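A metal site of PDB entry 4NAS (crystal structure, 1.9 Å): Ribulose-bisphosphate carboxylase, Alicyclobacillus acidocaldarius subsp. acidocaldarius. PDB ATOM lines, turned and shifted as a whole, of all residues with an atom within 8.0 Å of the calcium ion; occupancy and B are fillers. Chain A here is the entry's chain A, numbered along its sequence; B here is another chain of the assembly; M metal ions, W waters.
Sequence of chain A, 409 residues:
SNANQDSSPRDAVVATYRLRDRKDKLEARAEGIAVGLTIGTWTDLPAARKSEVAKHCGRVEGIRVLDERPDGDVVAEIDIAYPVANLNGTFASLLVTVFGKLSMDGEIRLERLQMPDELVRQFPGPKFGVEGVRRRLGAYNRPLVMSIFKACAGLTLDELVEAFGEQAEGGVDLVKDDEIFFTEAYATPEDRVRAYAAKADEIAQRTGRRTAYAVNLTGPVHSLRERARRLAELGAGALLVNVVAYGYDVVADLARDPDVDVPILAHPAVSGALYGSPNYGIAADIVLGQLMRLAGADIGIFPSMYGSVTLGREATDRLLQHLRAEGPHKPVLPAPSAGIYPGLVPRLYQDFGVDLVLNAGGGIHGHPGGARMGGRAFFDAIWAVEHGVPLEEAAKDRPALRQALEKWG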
ATOM      1  N   ILE A 148     -10.498  10.269 -15.092  1.00  0.00           N
ATOM      2  CA  ILE A 148     -10.500  11.675 -15.493  1.00  0.00           C
ATOM      3  C   ILE A 148     -11.935  12.180 -15.544  1.00  0.00           C
ATOM      4  O   ILE A 148     -12.809  11.485 -16.030  1.00  0.00           O
ATOM      5  CB  ILE A 148      -9.922  11.818 -16.925  1.00  0.00           C
ATOM      6  CG1 ILE A 148      -8.606  11.048 -17.052  1.00  0.00           C
ATOM      7  CG2 ILE A 148      -9.795  13.286 -17.318  1.00  0.00           C
ATOM      8  CD1 ILE A 148      -8.342  10.496 -18.454  1.00  0.00           C
ATOM      9  N   PHE A 149     -12.168  13.375 -15.016  1.00  0.00           N
ATOM     10  CA  PHE A 149     -13.466  14.035 -15.187  1.00  0.00           C
ATOM     11  C   PHE A 149     -13.829  14.096 -16.658  1.00  0.00           C
ATOM     12  O   PHE A 149     -12.999  14.440 -17.526  1.00  0.00           O
ATOM     13  CB  PHE A 149     -13.434  15.463 -14.647  1.00  0.00           C
ATOM     14  CG  PHE A 149     -13.921  15.604 -13.240  1.00  0.00           C
ATOM     15  CD1 PHE A 149     -13.063  15.390 -12.160  1.00  0.00           C
ATOM     16  CD2 PHE A 149     -15.225  15.997 -12.983  1.00  0.00           C
ATOM     17  CE1 PHE A 149     -13.526  15.536 -10.845  1.00  0.00           C
ATOM     18  CE2 PHE A 149     -15.693  16.156 -11.678  1.00  0.00           C
ATOM     19  CZ  PHE A 149     -14.829  15.935 -10.609  1.00  0.00           C
ATOM     20  N   KCX A 176      -8.559  12.917 -11.681  1.00  0.00           N
ATOM     21  CA  KCX A 176      -7.883  14.105 -12.100  1.00  0.00           C
ATOM     22  CB  KCX A 176      -6.659  13.790 -12.972  1.00  0.00           C
ATOM     23  CG  KCX A 176      -7.018  13.298 -14.364  1.00  0.00           C
ATOM     24  CD  KCX A 176      -5.755  13.002 -15.249  1.00  0.00           C
ATOM     25  CE  KCX A 176      -5.309  14.229 -16.109  1.00  0.00           C
ATOM     26  NZ  KCX A 176      -6.386  14.901 -16.817  1.00  0.00           N
ATOM     27  C   KCX A 176      -8.854  15.063 -12.829  1.00  0.00           C
ATOM     28  O   KCX A 176      -9.751  14.600 -13.563  1.00  0.00           O
ATOM     29  CX  KCX A 176      -6.456  14.600 -18.231  1.00  0.00           C
ATOM     30  OQ1 KCX A 176      -5.524  14.006 -18.882  1.00  0.00           O
ATOM     31  OQ2 KCX A 176      -7.499  14.952 -18.863  1.00  0.00           O
ATOM     32  N   ASP A 177      -8.694  16.367 -12.627  1.00  0.00           N
ATOM     33  CA  ASP A 177      -9.356  17.354 -13.481  1.00  0.00           C
ATOM     34  C   ASP A 177      -9.025  17.050 -14.950  1.00  0.00           C
ATOM     35  O   ASP A 177      -7.962  16.498 -15.256  1.00  0.00           O
ATOM     36  CB  ASP A 177      -8.836  18.759 -13.177  1.00  0.00           C
ATOM     37  CG  ASP A 177      -9.495  19.371 -11.969  1.00  0.00           C
ATOM     38  OD1 ASP A 177     -10.540  18.848 -11.511  1.00  0.00           O
ATOM     39  OD2 ASP A 177      -8.963  20.403 -11.491  1.00  0.00           O
ATOM     40  N   ASP A 178      -9.929  17.405 -15.854  1.00  0.00           N
ATOM     41  CA  ASP A 178      -9.604  17.454 -17.275  1.00  0.00           C
ATOM     42  C   ASP A 178      -8.544  18.580 -17.414  1.00  0.00           C
ATOM     43  O   ASP A 178      -8.656  19.611 -16.726  1.00  0.00           O
ATOM     44  CB  ASP A 178     -10.853  17.787 -18.075  1.00  0.00           C
ATOM     45  CG  ASP A 178     -10.766  17.355 -19.542  1.00  0.00           C
ATOM     46  OD1 ASP A 178      -9.679  16.878 -19.958  1.00  0.00           O
ATOM     47  OD2 ASP A 178     -11.780  17.497 -20.286  1.00  0.00           O
ATOM     48  N   GLU A 179      -7.521  18.410 -18.252  1.00  0.00           N
ATOM     49  CA  GLU A 179      -6.439  19.412 -18.248  1.00  0.00           C
ATOM     50  C   GLU A 179      -6.866  20.729 -18.860  1.00  0.00           C
ATOM     51  O   GLU A 179      -6.137  21.727 -18.793  1.00  0.00           O
ATOM     52  CB  GLU A 179      -5.145  18.885 -18.907  1.00  0.00           C
ATOM     53  CG  GLU A 179      -5.105  18.994 -20.429  1.00  0.00           C
ATOM     54  CD  GLU A 179      -6.050  18.023 -21.137  1.00  0.00           C
ATOM     55  OE1 GLU A 179      -6.505  17.054 -20.491  1.00  0.00           O
ATOM     56  OE2 GLU A 179      -6.343  18.233 -22.341  1.00  0.00           O
ATOM     57  N   ILE A 180      -8.064  20.746 -19.452  1.00  0.00           N
ATOM     58  CA  ILE A 180      -8.577  21.971 -20.061  1.00  0.00           C
ATOM     59  C   ILE A 180      -9.401  22.815 -19.102  1.00  0.00           C
ATOM     60  O   ILE A 180      -9.953  23.840 -19.510  1.00  0.00           O
ATOM     61  CB  ILE A 180      -9.404  21.685 -21.317  1.00  0.00           C
ATOM     62  CG1 ILE A 180     -10.581  20.763 -20.966  1.00  0.00           C
ATOM     63  CG2 ILE A 180      -8.516  21.091 -22.426  1.00  0.00           C
ATOM     64  CD1 ILE A 180     -11.416  20.416 -22.151  1.00  0.00           C
ATOM     65  N   PHE A 181      -9.476  22.405 -17.841  1.00  0.00           N
ATOM     66  CA  PHE A 181     -10.323  23.098 -16.849  1.00  0.00           C
ATOM     67  C   PHE A 181      -9.599  24.340 -16.314  1.00  0.00           C
ATOM     68  O   PHE A 181      -8.737  24.249 -15.437  1.00  0.00           O
ATOM     69  CB  PHE A 181     -10.670  22.162 -15.693  1.00  0.00           C
ATOM     70  CG  PHE A 181     -11.864  22.602 -14.844  1.00  0.00           C
ATOM     71  CD1 PHE A 181     -12.635  23.698 -15.206  1.00  0.00           C
ATOM     72  CD2 PHE A 181     -12.212  21.880 -13.701  1.00  0.00           C
ATOM     73  CE1 PHE A 181     -13.739  24.089 -14.420  1.00  0.00           C
ATOM     74  CE2 PHE A 181     -13.298  22.266 -12.930  1.00  0.00           C
ATOM     75  CZ  PHE A 181     -14.060  23.371 -13.285  1.00  0.00           C
ATOM     76  N   LEU A 240      -2.051  18.560 -10.991  1.00  0.00           N
ATOM     77  CA  LEU A 240      -1.974  18.350 -12.427  1.00  0.00           C
ATOM     78  C   LEU A 240      -1.350  19.581 -13.067  1.00  0.00           C
ATOM     79  O   LEU A 240      -1.826  20.697 -12.899  1.00  0.00           O
ATOM     80  CB  LEU A 240      -3.375  18.139 -12.998  1.00  0.00           C
ATOM     81  CG  LEU A 240      -3.581  18.083 -14.514  1.00  0.00           C
ATOM     82  CD1 LEU A 240      -2.794  16.955 -15.128  1.00  0.00           C
ATOM     83  CD2 LEU A 240      -5.087  17.937 -14.841  1.00  0.00           C
ATOM     84  N   HIS A 267       1.052  16.592 -17.331  1.00  0.00           N
ATOM     85  CA  HIS A 267       0.246  16.398 -18.530  1.00  0.00           C
ATOM     86  C   HIS A 267       1.037  16.851 -19.744  1.00  0.00           C
ATOM     87  O   HIS A 267       1.694  17.894 -19.702  1.00  0.00           O
ATOM     88  CB  HIS A 267      -1.092  17.139 -18.457  1.00  0.00           C
ATOM     89  CG  HIS A 267      -1.987  16.856 -19.619  1.00  0.00           C
ATOM     90  ND1 HIS A 267      -3.005  15.924 -19.577  1.00  0.00           N
ATOM     91  CD2 HIS A 267      -1.945  17.310 -20.896  1.00  0.00           C
ATOM     92  CE1 HIS A 267      -3.575  15.844 -20.762  1.00  0.00           C
ATOM     93  NE2 HIS A 267      -2.965  16.681 -21.587  1.00  0.00           N
ATOM     94  N   ILE A 301       2.228  11.494 -17.887  1.00  0.00           N
ATOM     95  CA  ILE A 301       1.220  11.119 -18.871  1.00  0.00           C
ATOM     96  C   ILE A 301       1.806  11.265 -20.274  1.00  0.00           C
ATOM     97  O   ILE A 301       2.392  12.296 -20.588  1.00  0.00           O
ATOM     98  CB  ILE A 301      -0.017  12.042 -18.763  1.00  0.00           C
ATOM     99  CG1 ILE A 301      -0.769  11.789 -17.435  1.00  0.00           C
ATOM    100  CG2 ILE A 301      -0.976  11.799 -19.943  1.00  0.00           C
ATOM    101  CD1 ILE A 301      -1.739  12.888 -17.089  1.00  0.00           C
ATOM    102  N   ASN A 359      -4.650   4.813 -16.837  1.00  0.00           N
ATOM    103  CA  ASN A 359      -5.110   6.174 -17.025  1.00  0.00           C
ATOM    104  C   ASN A 359      -6.324   6.119 -17.920  1.00  0.00           C
ATOM    105  O   ASN A 359      -6.209   6.129 -19.139  1.00  0.00           O
ATOM    106  CB  ASN A 359      -3.981   6.983 -17.675  1.00  0.00           C
ATOM    107  CG  ASN A 359      -4.377   8.400 -18.023  1.00  0.00           C
ATOM    108  OD1 ASN A 359      -5.418   8.905 -17.614  1.00  0.00           O
ATOM    109  ND2 ASN A 359      -3.510   9.071 -18.780  1.00  0.00           N
ATOM    110  N   GLY A 361     -10.054   7.446 -19.259  1.00  0.00           N
ATOM    111  CA  GLY A 361     -11.123   8.414 -19.383  1.00  0.00           C
ATOM    112  C   GLY A 361     -12.375   7.715 -19.862  1.00  0.00           C
ATOM    113  O   GLY A 361     -13.266   7.344 -19.058  1.00  0.00           O
ATOM    114  N   GLY B  36     -15.113  18.159 -27.098  1.00  0.00           N
ATOM    115  CA  GLY B  36     -14.152  17.592 -26.168  1.00  0.00           C
ATOM    116  C   GLY B  36     -13.175  18.575 -25.544  1.00  0.00           C
ATOM    117  O   GLY B  36     -12.710  18.363 -24.432  1.00  0.00           O
ATOM    118  N   LEU B  37     -12.822  19.618 -26.273  1.00  0.00           N
ATOM    119  CA  LEU B  37     -11.869  20.619 -25.769  1.00  0.00           C
ATOM    120  C   LEU B  37     -12.558  21.834 -25.141  1.00  0.00           C
ATOM    121  O   LEU B  37     -11.912  22.833 -24.861  1.00  0.00           O
ATOM    122  CB  LEU B  37     -10.939  21.090 -26.890  1.00  0.00           C
ATOM    123  CG  LEU B  37     -10.094  19.985 -27.502  1.00  0.00           C
ATOM    124  CD1 LEU B  37      -9.175  20.559 -28.567  1.00  0.00           C
ATOM    125  CD2 LEU B  37      -9.299  19.239 -26.430  1.00  0.00           C
ATOM    126  N   VAL B  96      -3.205  25.360 -24.036  1.00  0.00           N
ATOM    127  CA  VAL B  96      -3.672  24.006 -23.659  1.00  0.00           C
ATOM    128  C   VAL B  96      -5.039  23.733 -24.266  1.00  0.00           C
ATOM    129  O   VAL B  96      -5.363  22.589 -24.624  1.00  0.00           O
ATOM    130  CB  VAL B  96      -3.770  23.860 -22.148  1.00  0.00           C
ATOM    131  CG1 VAL B  96      -4.621  22.593 -21.773  1.00  0.00           C
ATOM    132  CG2 VAL B  96      -2.400  23.756 -21.513  1.00  0.00           C
ATOM    133  N   LYS B 101      -3.779  18.872 -26.003  1.00  0.00           N
ATOM    134  CA  LYS B 101      -3.904  17.488 -26.416  1.00  0.00           C
ATOM    135  C   LYS B 101      -3.961  17.411 -27.942  1.00  0.00           C
ATOM    136  O   LYS B 101      -3.489  16.447 -28.522  1.00  0.00           O
ATOM    137  CB  LYS B 101      -5.166  16.870 -25.832  1.00  0.00           C
ATOM    138  CG  LYS B 101      -5.353  15.421 -26.230  1.00  0.00           C
ATOM    139  CD  LYS B 101      -6.797  15.105 -26.547  1.00  0.00           C
ATOM    140  CE  LYS B 101      -7.614  14.952 -25.295  1.00  0.00           C
ATOM    141  NZ  LYS B 101      -9.091  14.957 -25.563  1.00  0.00           N
HETATM  142 CA    CA M   1      -8.032  15.455 -20.971  1.00  0.00          CA
HETATM  143  O   HOH W   1      -6.150  14.023 -21.445  1.00  0.00           O
HETATM  144  O   HOH W   2      -8.451  16.694 -22.919  1.00  0.00           O
HETATM  145  O   HOH W   3      -9.800  13.776 -21.058  1.00  0.00           O
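O of KCX 176 lies within hydrogen-bond range of the backbone NH (N) of Phe 149 (3.1 Å). OQ1 of KCX 176 sits at hydrogen-bond distance from a ring nitrogen (ND1) of His 267.
Three residues have an atom within 4 Å of the calcium ion: KCX 176, Asp 178 and Glu 179. Along chain A the residues within 4 Å of the calcium ion span positions 176 to 179.
The calcium ion is bound by OQ2 of KCX 176 (2.2 Å), the side-chain carboxylate (OE1) of Glu 179 (2.3 Å), water W2 (2.3 Å), the side-chain carboxylate (OD1) of Asp 178 (2.4 Å), water W1 (2.4 Å) and water W3 (2.4 Å).
Water W2 lies within hydrogen-bond range of the side-chain carboxylate of Glu 179 (2.7 Å) and the side-chain amino group of Lys 101 of chain B (3.2 Å).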
